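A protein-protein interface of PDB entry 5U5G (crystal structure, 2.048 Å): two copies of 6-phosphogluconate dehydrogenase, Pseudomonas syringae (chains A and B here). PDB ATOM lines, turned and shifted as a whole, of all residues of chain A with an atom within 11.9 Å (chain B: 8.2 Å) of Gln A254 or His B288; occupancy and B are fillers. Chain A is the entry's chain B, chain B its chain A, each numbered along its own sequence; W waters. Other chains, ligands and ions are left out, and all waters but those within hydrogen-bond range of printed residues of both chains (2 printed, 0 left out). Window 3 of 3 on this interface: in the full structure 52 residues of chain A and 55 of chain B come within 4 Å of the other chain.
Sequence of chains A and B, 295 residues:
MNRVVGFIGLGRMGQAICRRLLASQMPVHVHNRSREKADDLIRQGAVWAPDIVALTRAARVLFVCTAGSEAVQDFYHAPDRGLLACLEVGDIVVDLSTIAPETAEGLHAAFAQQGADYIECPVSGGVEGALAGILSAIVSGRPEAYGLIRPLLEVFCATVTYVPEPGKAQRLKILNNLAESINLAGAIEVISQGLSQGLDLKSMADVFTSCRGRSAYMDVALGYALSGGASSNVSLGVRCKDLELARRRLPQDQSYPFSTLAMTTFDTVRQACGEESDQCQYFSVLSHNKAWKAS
NE2 of Gln B193 is in hydrogen-bond range of OG of Ser A259.
The backbone carbonyl oxygen (O) of Leu B286 sits at hydrogen-bond distance from the side-chain amide nitrogen (NE2) of Gln A254, 2.9 Å away.
Leu A178 touches Gln B193 (CD1 to NE2, 3.8 Å).
CD2 of Leu A250 touches OE1 of Gln B193, 3.3 Å away.
Gln A254 touches His B288 (NE2 to ND1, 3.8 Å).
Ser A255 touches Leu B286 (O to CD1, 3.7 Å).
Gln B193 touches Tyr A256.
Tyr A256 touches Leu B286.
OH of Tyr B282 touches CD of Pro A257, 3.6 Å away.
Of chain B, only Leu B286 and His B288 come within 4 Å of Gln A254.
His B288 touches one residue of chain A.
Ser A255 touches just one residue of chain B: Leu B286.
No residue of chain A comes within 4 Å of Ser B284.
Val B285 touches none of the printed residues of chain A.
Of the printed residues of chain B, Leu A250 touches Gln B193 (3.3 Å).
Of the printed residues of chain B, Pro A257 touches Tyr B282.
Printed residues of chain B within 4 Å of Ser A259: Gln B193.
Of the printed residues of chain B, Leu A178 touches Gln B193.
Printed residues of chain B within 4 Å of Tyr A256: Gln B193 (3.6 Å) and Leu B286 (3.97 Å).
Thr A260 touches none of the printed residues of chain B.
The nearest residue of chain A that does not touch His B288 is Asp A253 (6.6 Å).
The nearest printed residue of chain A that does not touch Gln B193 is Ala A246 (5.0 Å).
No position is printed for both chains.
Water W2 lies within hydrogen-bond range of the backbone carbonyl oxygen (O) of Arg A249 (2.8 Å) and the side-chain amide oxygen (OE1) of Gln B193 (3.0 Å).
Water W1 bridges the side-chain amide oxygen of Gln B193 and the backbone carbonyl oxygen of Ala A246.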
ATOM      1  N   LEU A 178       3.736  34.765 -19.263  1.00  0.00           N
ATOM      2  CA  LEU A 178       3.568  34.379 -20.662  1.00  0.00           C
ATOM      3  C   LEU A 178       2.096  34.355 -21.036  1.00  0.00           C
ATOM      4  O   LEU A 178       1.703  34.878 -22.084  1.00  0.00           O
ATOM      5  CB  LEU A 178       4.191  33.005 -20.899  1.00  0.00           C
ATOM      6  CG  LEU A 178       5.054  32.754 -22.127  1.00  0.00           C
ATOM      7  CD1 LEU A 178       5.092  31.258 -22.416  1.00  0.00           C
ATOM      8  CD2 LEU A 178       4.621  33.557 -23.343  1.00  0.00           C
ATOM      9  N   ALA A 246      11.108  33.721 -20.349  1.00  0.00           N
ATOM     10  CA  ALA A 246      10.350  32.594 -20.882  1.00  0.00           C
ATOM     11  C   ALA A 246      11.018  32.018 -22.118  1.00  0.00           C
ATOM     12  O   ALA A 246      11.074  30.795 -22.281  1.00  0.00           O
ATOM     13  CB  ALA A 246       8.919  33.020 -21.217  1.00  0.00           C
ATOM     14  N   ARG A 247      11.518  32.889 -23.003  1.00  0.00           N
ATOM     15  CA  ARG A 247      12.170  32.425 -24.224  1.00  0.00           C
ATOM     16  C   ARG A 247      13.342  31.515 -23.910  1.00  0.00           C
ATOM     17  O   ARG A 247      13.540  30.491 -24.573  1.00  0.00           O
ATOM     18  CB  ARG A 247      12.654  33.613 -25.061  1.00  0.00           C
ATOM     19  CG  ARG A 247      12.904  33.249 -26.521  1.00  0.00           C
ATOM     20  CD  ARG A 247      13.586  34.377 -27.301  1.00  0.00           C
ATOM     21  NE  ARG A 247      14.760  34.886 -26.599  1.00  0.00           N
ATOM     22  CZ  ARG A 247      15.991  34.407 -26.764  1.00  0.00           C
ATOM     23  NH1 ARG A 247      16.207  33.402 -27.601  1.00  0.00           N
ATOM     24  NH2 ARG A 247      17.014  34.915 -26.085  1.00  0.00           N
ATOM     25  N   ARG A 248      14.137  31.881 -22.910  1.00  0.00           N
ATOM     26  CA  ARG A 248      15.298  31.102 -22.525  1.00  0.00           C
ATOM     27  C   ARG A 248      14.922  29.742 -21.960  1.00  0.00           C
ATOM     28  O   ARG A 248      15.803  28.895 -21.797  1.00  0.00           O
ATOM     29  CB  ARG A 248      16.125  31.890 -21.511  1.00  0.00           C
ATOM     30  CG  ARG A 248      16.945  33.048 -22.125  1.00  0.00           C
ATOM     31  CD  ARG A 248      17.720  33.799 -21.043  1.00  0.00           C
ATOM     32  NE  ARG A 248      17.765  32.994 -19.833  1.00  0.00           N
ATOM     33  CZ  ARG A 248      17.826  33.475 -18.593  1.00  0.00           C
ATOM     34  NH1 ARG A 248      17.892  34.787 -18.366  1.00  0.00           N
ATOM     35  NH2 ARG A 248      17.838  32.636 -17.564  1.00  0.00           N
ATOM     36  N   ARG A 249      13.646  29.507 -21.661  1.00  0.00           N
ATOM     37  CA  ARG A 249      13.216  28.228 -21.122  1.00  0.00           C
ATOM     38  C   ARG A 249      12.447  27.394 -22.132  1.00  0.00           C
ATOM     39  O   ARG A 249      11.957  26.312 -21.780  1.00  0.00           O
ATOM     40  CB  ARG A 249      12.387  28.449 -19.853  1.00  0.00           C
ATOM     41  CG  ARG A 249      13.192  29.190 -18.780  1.00  0.00           C
ATOM     42  CD  ARG A 249      12.438  29.351 -17.475  1.00  0.00           C
ATOM     43  NE  ARG A 249      12.102  28.071 -16.870  1.00  0.00           N
ATOM     44  CZ  ARG A 249      12.943  27.314 -16.166  1.00  0.00           C
ATOM     45  NH1 ARG A 249      14.207  27.693 -15.970  1.00  0.00           N
ATOM     46  NH2 ARG A 249      12.511  26.162 -15.658  1.00  0.00           N
ATOM     47  N   LEU A 250      12.332  27.863 -23.373  1.00  0.00           N
ATOM     48  CA  LEU A 250      11.739  27.045 -24.423  1.00  0.00           C
ATOM     49  C   LEU A 250      12.643  25.851 -24.729  1.00  0.00           C
ATOM     50  O   LEU A 250      13.868  25.995 -24.751  1.00  0.00           O
ATOM     51  CB  LEU A 250      11.533  27.865 -25.696  1.00  0.00           C
ATOM     52  CG  LEU A 250      10.511  28.994 -25.626  1.00  0.00           C
ATOM     53  CD1 LEU A 250      10.558  29.797 -26.923  1.00  0.00           C
ATOM     54  CD2 LEU A 250       9.114  28.423 -25.361  1.00  0.00           C
ATOM     55  N   PRO A 251      12.076  24.673 -24.978  1.00  0.00           N
ATOM     56  CA  PRO A 251      12.889  23.526 -25.394  1.00  0.00           C
ATOM     57  C   PRO A 251      13.291  23.637 -26.860  1.00  0.00           C
ATOM     58  O   PRO A 251      12.801  24.477 -27.618  1.00  0.00           O
ATOM     59  CB  PRO A 251      11.947  22.341 -25.175  1.00  0.00           C
ATOM     60  CG  PRO A 251      10.610  22.906 -25.466  1.00  0.00           C
ATOM     61  CD  PRO A 251      10.641  24.342 -24.959  1.00  0.00           C
ATOM     62  N   GLN A 252      14.208  22.759 -27.254  1.00  0.00           N
ATOM     63  CA  GLN A 252      14.666  22.741 -28.636  1.00  0.00           C
ATOM     64  C   GLN A 252      13.740  21.935 -29.539  1.00  0.00           C
ATOM     65  O   GLN A 252      13.641  22.226 -30.736  1.00  0.00           O
ATOM     66  CB  GLN A 252      16.083  22.166 -28.709  1.00  0.00           C
ATOM     67  CG  GLN A 252      17.195  23.100 -28.256  1.00  0.00           C
ATOM     68  CD  GLN A 252      17.682  24.001 -29.377  1.00  0.00           C
ATOM     69  OE1 GLN A 252      16.890  24.686 -30.031  1.00  0.00           O
ATOM     70  NE2 GLN A 252      18.990  23.992 -29.618  1.00  0.00           N
ATOM     71  N   ASP A 253      13.046  20.944 -28.987  1.00  0.00           N
ATOM     72  CA  ASP A 253      12.379  19.923 -29.783  1.00  0.00           C
ATOM     73  C   ASP A 253      10.889  20.175 -29.998  1.00  0.00           C
ATOM     74  O   ASP A 253      10.248  19.387 -30.700  1.00  0.00           O
ATOM     75  CB  ASP A 253      12.559  18.545 -29.135  1.00  0.00           C
ATOM     76  CG  ASP A 253      11.623  18.324 -27.945  1.00  0.00           C
ATOM     77  OD1 ASP A 253      11.441  19.259 -27.126  1.00  0.00           O
ATOM     78  OD2 ASP A 253      11.060  17.206 -27.834  1.00  0.00           O
ATOM     79  N   GLN A 254      10.312  21.221 -29.409  1.00  0.00           N
ATOM     80  CA  GLN A 254       8.877  21.424 -29.550  1.00  0.00           C
ATOM     81  C   GLN A 254       8.576  22.898 -29.768  1.00  0.00           C
ATOM     82  O   GLN A 254       9.164  23.766 -29.119  1.00  0.00           O
ATOM     83  CB  GLN A 254       8.104  20.898 -28.341  1.00  0.00           C
ATOM     84  CG  GLN A 254       6.614  21.043 -28.528  1.00  0.00           C
ATOM     85  CD  GLN A 254       6.151  20.318 -29.781  1.00  0.00           C
ATOM     86  OE1 GLN A 254       5.820  20.941 -30.800  1.00  0.00           O
ATOM     87  NE2 GLN A 254       6.159  18.988 -29.724  1.00  0.00           N
ATOM     88  N   SER A 255       7.656  23.164 -30.693  1.00  0.00           N
ATOM     89  CA  SER A 255       7.210  24.514 -30.997  1.00  0.00           C
ATOM     90  C   SER A 255       6.080  24.926 -30.069  1.00  0.00           C
ATOM     91  O   SER A 255       5.180  24.134 -29.762  1.00  0.00           O
ATOM     92  CB  SER A 255       6.731  24.608 -32.444  1.00  0.00           C
ATOM     93  OG  SER A 255       7.836  24.610 -33.325  1.00  0.00           O
ATOM     94  N   TYR A 256       6.112  26.181 -29.651  1.00  0.00           N
ATOM     95  CA  TYR A 256       5.022  26.788 -28.897  1.00  0.00           C
ATOM     96  C   TYR A 256       4.655  28.097 -29.589  1.00  0.00           C
ATOM     97  O   TYR A 256       5.107  29.174 -29.182  1.00  0.00           O
ATOM     98  CB  TYR A 256       5.420  26.984 -27.439  1.00  0.00           C
ATOM     99  CG  TYR A 256       5.592  25.674 -26.701  1.00  0.00           C
ATOM    100  CD1 TYR A 256       4.484  25.000 -26.196  1.00  0.00           C
ATOM    101  CD2 TYR A 256       6.858  25.108 -26.509  1.00  0.00           C
ATOM    102  CE1 TYR A 256       4.616  23.805 -25.526  1.00  0.00           C
ATOM    103  CE2 TYR A 256       7.004  23.888 -25.827  1.00  0.00           C
ATOM    104  CZ  TYR A 256       5.877  23.248 -25.342  1.00  0.00           C
ATOM    105  OH  TYR A 256       5.987  22.053 -24.662  1.00  0.00           O
ATOM    106  N   PRO A 257       3.811  28.040 -30.627  1.00  0.00           N
ATOM    107  CA  PRO A 257       3.675  29.204 -31.530  1.00  0.00           C
ATOM    108  C   PRO A 257       3.094  30.453 -30.880  1.00  0.00           C
ATOM    109  O   PRO A 257       3.579  31.553 -31.160  1.00  0.00           O
ATOM    110  CB  PRO A 257       2.762  28.670 -32.647  1.00  0.00           C
ATOM    111  CG  PRO A 257       2.881  27.172 -32.556  1.00  0.00           C
ATOM    112  CD  PRO A 257       3.053  26.871 -31.102  1.00  0.00           C
ATOM    113  N   PHE A 258       2.064  30.329 -30.033  1.00  0.00           N
ATOM    114  CA  PHE A 258       1.540  31.509 -29.341  1.00  0.00           C
ATOM    115  C   PHE A 258       2.571  32.122 -28.398  1.00  0.00           C
ATOM    116  O   PHE A 258       2.661  33.353 -28.285  1.00  0.00           O
ATOM    117  CB  PHE A 258       0.259  31.154 -28.584  1.00  0.00           C
ATOM    118  CG  PHE A 258      -0.963  31.146 -29.457  1.00  0.00           C
ATOM    119  CD1 PHE A 258      -1.319  30.007 -30.155  1.00  0.00           C
ATOM    120  CD2 PHE A 258      -1.747  32.292 -29.593  1.00  0.00           C
ATOM    121  CE1 PHE A 258      -2.440  30.006 -30.988  1.00  0.00           C
ATOM    122  CE2 PHE A 258      -2.863  32.295 -30.413  1.00  0.00           C
ATOM    123  CZ  PHE A 258      -3.208  31.144 -31.116  1.00  0.00           C
ATOM    124  N   SER A 259       3.346  31.279 -27.704  1.00  0.00           N
ATOM    125  CA  SER A 259       4.388  31.762 -26.799  1.00  0.00           C
ATOM    126  C   SER A 259       5.464  32.520 -27.562  1.00  0.00           C
ATOM    127  O   SER A 259       5.890  33.607 -27.152  1.00  0.00           O
ATOM    128  CB  SER A 259       5.014  30.582 -26.049  1.00  0.00           C
ATOM    129  OG  SER A 259       4.027  29.824 -25.384  1.00  0.00           O
ATOM    130  N   THR A 260       5.922  31.944 -28.674  1.00  0.00           N
ATOM    131  CA  THR A 260       6.923  32.588 -29.512  1.00  0.00           C
ATOM    132  C   THR A 260       6.382  33.863 -30.158  1.00  0.00           C
ATOM    133  O   THR A 260       7.095  34.870 -30.242  1.00  0.00           O
ATOM    134  CB  THR A 260       7.408  31.584 -30.566  1.00  0.00           C
ATOM    135  OG1 THR A 260       8.239  30.612 -29.920  1.00  0.00           O
ATOM    136  CG2 THR A 260       8.212  32.279 -31.645  1.00  0.00           C
ATOM    137  N   LEU A 261       5.125  33.852 -30.602  1.00  0.00           N
ATOM    138  CA  LEU A 261       4.537  35.065 -31.163  1.00  0.00           C
ATOM    139  C   LEU A 261       4.468  36.185 -30.125  1.00  0.00           C
ATOM    140  O   LEU A 261       4.704  37.355 -30.446  1.00  0.00           O
ATOM    141  CB  LEU A 261       3.152  34.773 -31.733  1.00  0.00           C
ATOM    142  CG  LEU A 261       2.459  35.982 -32.375  1.00  0.00           C
ATOM    143  CD1 LEU A 261       3.274  36.514 -33.544  1.00  0.00           C
ATOM    144  CD2 LEU A 261       1.024  35.636 -32.838  1.00  0.00           C
ATOM    145  N   MET A 263       6.566  36.612 -27.606  1.00  0.00           N
ATOM    146  CA  MET A 263       7.934  37.109 -27.445  1.00  0.00           C
ATOM    147  C   MET A 263       8.330  38.043 -28.586  1.00  0.00           C
ATOM    148  O   MET A 263       8.888  39.122 -28.345  1.00  0.00           O
ATOM    149  CB  MET A 263       8.919  35.942 -27.345  1.00  0.00           C
ATOM    150  CG  MET A 263       8.705  35.068 -26.119  1.00  0.00           C
ATOM    151  SD  MET A 263       9.241  33.366 -26.352  1.00  0.00           S
ATOM    152  CE  MET A 263       8.572  32.595 -24.868  1.00  0.00           C
ATOM    153  N   SER B 192       1.431  23.236 -20.721  1.00  0.00           N
ATOM    154  CA  SER B 192       2.263  22.174 -21.283  1.00  0.00           C
ATOM    155  C   SER B 192       3.734  22.403 -20.968  1.00  0.00           C
ATOM    156  O   SER B 192       4.447  21.475 -20.564  1.00  0.00           O
ATOM    157  CB  SER B 192       2.053  22.077 -22.793  1.00  0.00           C
ATOM    158  OG  SER B 192       0.710  21.734 -23.067  1.00  0.00           O
ATOM    159  N   GLN B 193       4.207  23.633 -21.175  1.00  0.00           N
ATOM    160  CA  GLN B 193       5.585  23.968 -20.837  1.00  0.00           C
ATOM    161  C   GLN B 193       5.860  23.718 -19.363  1.00  0.00           C
ATOM    162  O   GLN B 193       6.904  23.160 -19.007  1.00  0.00           O
ATOM    163  CB  GLN B 193       5.870  25.430 -21.200  1.00  0.00           C
ATOM    164  CG  GLN B 193       5.878  25.655 -22.693  1.00  0.00           C
ATOM    165  CD  GLN B 193       6.070  27.108 -23.076  1.00  0.00           C
ATOM    166  OE1 GLN B 193       7.143  27.686 -22.853  1.00  0.00           O
ATOM    167  NE2 GLN B 193       5.035  27.707 -23.672  1.00  0.00           N
ATOM    168  N   SER B 196       6.436  20.072 -18.806  1.00  0.00           N
ATOM    169  CA  SER B 196       7.746  19.693 -19.322  1.00  0.00           C
ATOM    170  C   SER B 196       8.860  20.202 -18.427  1.00  0.00           C
ATOM    171  O   SER B 196       9.922  19.573 -18.344  1.00  0.00           O
ATOM    172  CB  SER B 196       7.942  20.231 -20.740  1.00  0.00           C
ATOM    173  OG  SER B 196       7.022  19.620 -21.631  1.00  0.00           O
ATOM    174  N   THR B 268      -6.034  23.191 -37.624  1.00  0.00           N
ATOM    175  CA  THR B 268      -5.120  22.053 -37.658  1.00  0.00           C
ATOM    176  C   THR B 268      -5.485  21.006 -36.605  1.00  0.00           C
ATOM    177  O   THR B 268      -5.421  19.801 -36.873  1.00  0.00           O
ATOM    178  CB  THR B 268      -3.685  22.532 -37.462  1.00  0.00           C
ATOM    179  OG1 THR B 268      -3.380  23.532 -38.440  1.00  0.00           O
ATOM    180  CG2 THR B 268      -2.720  21.365 -37.633  1.00  0.00           C
ATOM    181  N   GLN B 281      -8.153  19.523 -27.164  1.00  0.00           N
ATOM    182  CA  GLN B 281      -7.229  18.541 -27.733  1.00  0.00           C
ATOM    183  C   GLN B 281      -5.986  19.174 -28.355  1.00  0.00           C
ATOM    184  O   GLN B 281      -5.084  18.445 -28.788  1.00  0.00           O
ATOM    185  CB  GLN B 281      -7.966  17.667 -28.751  1.00  0.00           C
ATOM    186  CG  GLN B 281      -8.589  16.418 -28.108  1.00  0.00           C
ATOM    187  CD  GLN B 281      -7.526  15.500 -27.520  1.00  0.00           C
ATOM    188  OE1 GLN B 281      -6.749  14.900 -28.256  1.00  0.00           O
ATOM    189  NE2 GLN B 281      -7.473  15.402 -26.196  1.00  0.00           N
ATOM    190  N   TYR B 282      -5.908  20.508 -28.407  1.00  0.00           N
ATOM    191  CA  TYR B 282      -4.624  21.151 -28.663  1.00  0.00           C
ATOM    192  C   TYR B 282      -3.532  20.595 -27.746  1.00  0.00           C
ATOM    193  O   TYR B 282      -2.369  20.526 -28.150  1.00  0.00           O
ATOM    194  CB  TYR B 282      -4.749  22.667 -28.480  1.00  0.00           C
ATOM    195  CG  TYR B 282      -3.516  23.471 -28.896  1.00  0.00           C
ATOM    196  CD1 TYR B 282      -2.772  23.119 -30.015  1.00  0.00           C
ATOM    197  CD2 TYR B 282      -3.136  24.611 -28.192  1.00  0.00           C
ATOM    198  CE1 TYR B 282      -1.661  23.875 -30.413  1.00  0.00           C
ATOM    199  CE2 TYR B 282      -2.028  25.371 -28.579  1.00  0.00           C
ATOM    200  CZ  TYR B 282      -1.305  25.005 -29.688  1.00  0.00           C
ATOM    201  OH  TYR B 282      -0.212  25.764 -30.056  1.00  0.00           O
ATOM    202  N   PHE B 283      -3.892  20.210 -26.510  1.00  0.00           N
ATOM    203  CA  PHE B 283      -2.950  19.568 -25.590  1.00  0.00           C
ATOM    204  C   PHE B 283      -2.226  18.413 -26.262  1.00  0.00           C
ATOM    205  O   PHE B 283      -0.997  18.335 -26.238  1.00  0.00           O
ATOM    206  CB  PHE B 283      -3.679  19.041 -24.343  1.00  0.00           C
ATOM    207  CG  PHE B 283      -3.680  19.990 -23.175  1.00  0.00           C
ATOM    208  CD1 PHE B 283      -2.488  20.388 -22.577  1.00  0.00           C
ATOM    209  CD2 PHE B 283      -4.882  20.460 -22.655  1.00  0.00           C
ATOM    210  CE1 PHE B 283      -2.503  21.263 -21.489  1.00  0.00           C
ATOM    211  CE2 PHE B 283      -4.908  21.313 -21.570  1.00  0.00           C
ATOM    212  CZ  PHE B 283      -3.717  21.720 -20.986  1.00  0.00           C
ATOM    213  N   SER B 284      -2.979  17.500 -26.874  1.00  0.00           N
ATOM    214  CA  SER B 284      -2.335  16.327 -27.447  1.00  0.00           C
ATOM    215  C   SER B 284      -1.636  16.650 -28.758  1.00  0.00           C
ATOM    216  O   SER B 284      -0.577  16.084 -29.041  1.00  0.00           O
ATOM    217  CB  SER B 284      -3.358  15.202 -27.632  1.00  0.00           C
ATOM    218  OG  SER B 284      -4.351  15.584 -28.565  1.00  0.00           O
ATOM    219  N   VAL B 285      -2.188  17.566 -29.558  1.00  0.00           N
ATOM    220  CA  VAL B 285      -1.513  17.976 -30.789  1.00  0.00           C
ATOM    221  C   VAL B 285      -0.189  18.642 -30.460  1.00  0.00           C
ATOM    222  O   VAL B 285       0.834  18.392 -31.111  1.00  0.00           O
ATOM    223  CB  VAL B 285      -2.416  18.909 -31.615  1.00  0.00           C
ATOM    224  CG1 VAL B 285      -1.620  19.567 -32.730  1.00  0.00           C
ATOM    225  CG2 VAL B 285      -3.601  18.138 -32.180  1.00  0.00           C
ATOM    226  N   LEU B 286      -0.186  19.484 -29.429  1.00  0.00           N
ATOM    227  CA  LEU B 286       1.034  20.174 -29.029  1.00  0.00           C
ATOM    228  C   LEU B 286       2.182  19.191 -28.829  1.00  0.00           C
ATOM    229  O   LEU B 286       3.271  19.372 -29.383  1.00  0.00           O
ATOM    230  CB  LEU B 286       0.767  20.976 -27.757  1.00  0.00           C
ATOM    231  CG  LEU B 286       1.539  22.259 -27.503  1.00  0.00           C
ATOM    232  CD1 LEU B 286       1.847  23.002 -28.788  1.00  0.00           C
ATOM    233  CD2 LEU B 286       0.690  23.102 -26.583  1.00  0.00           C
ATOM    234  N   SER B 287       1.945  18.128 -28.059  1.00  0.00           N
ATOM    235  CA  SER B 287       2.957  17.101 -27.842  1.00  0.00           C
ATOM    236  C   SER B 287       3.116  16.146 -29.024  1.00  0.00           C
ATOM    237  O   SER B 287       4.048  15.334 -29.005  1.00  0.00           O
ATOM    238  CB  SER B 287       2.634  16.311 -26.573  1.00  0.00           C
ATOM    239  OG  SER B 287       1.270  15.922 -26.534  1.00  0.00           O
ATOM    240  N   HIS B 288       2.249  16.235 -30.037  1.00  0.00           N
ATOM    241  CA  HIS B 288       2.270  15.396 -31.255  1.00  0.00           C
ATOM    242  C   HIS B 288       1.896  13.944 -30.980  1.00  0.00           C
ATOM    243  O   HIS B 288       1.187  13.639 -30.023  1.00  0.00           O
ATOM    244  CB  HIS B 288       3.642  15.445 -31.944  1.00  0.00           C
ATOM    245  CG  HIS B 288       3.745  16.478 -33.027  1.00  0.00           C
ATOM    246  ND1 HIS B 288       4.171  17.766 -32.785  1.00  0.00           N
ATOM    247  CD2 HIS B 288       3.488  16.409 -34.357  1.00  0.00           C
ATOM    248  CE1 HIS B 288       4.164  18.449 -33.915  1.00  0.00           C
ATOM    249  NE2 HIS B 288       3.758  17.649 -34.885  1.00  0.00           N
HETATM  250  O   HOH W   1       8.491  29.810 -21.432  1.00  0.00           O
HETATM  251  O   HOH W   2       9.219  25.872 -21.633  1.00  0.00           O
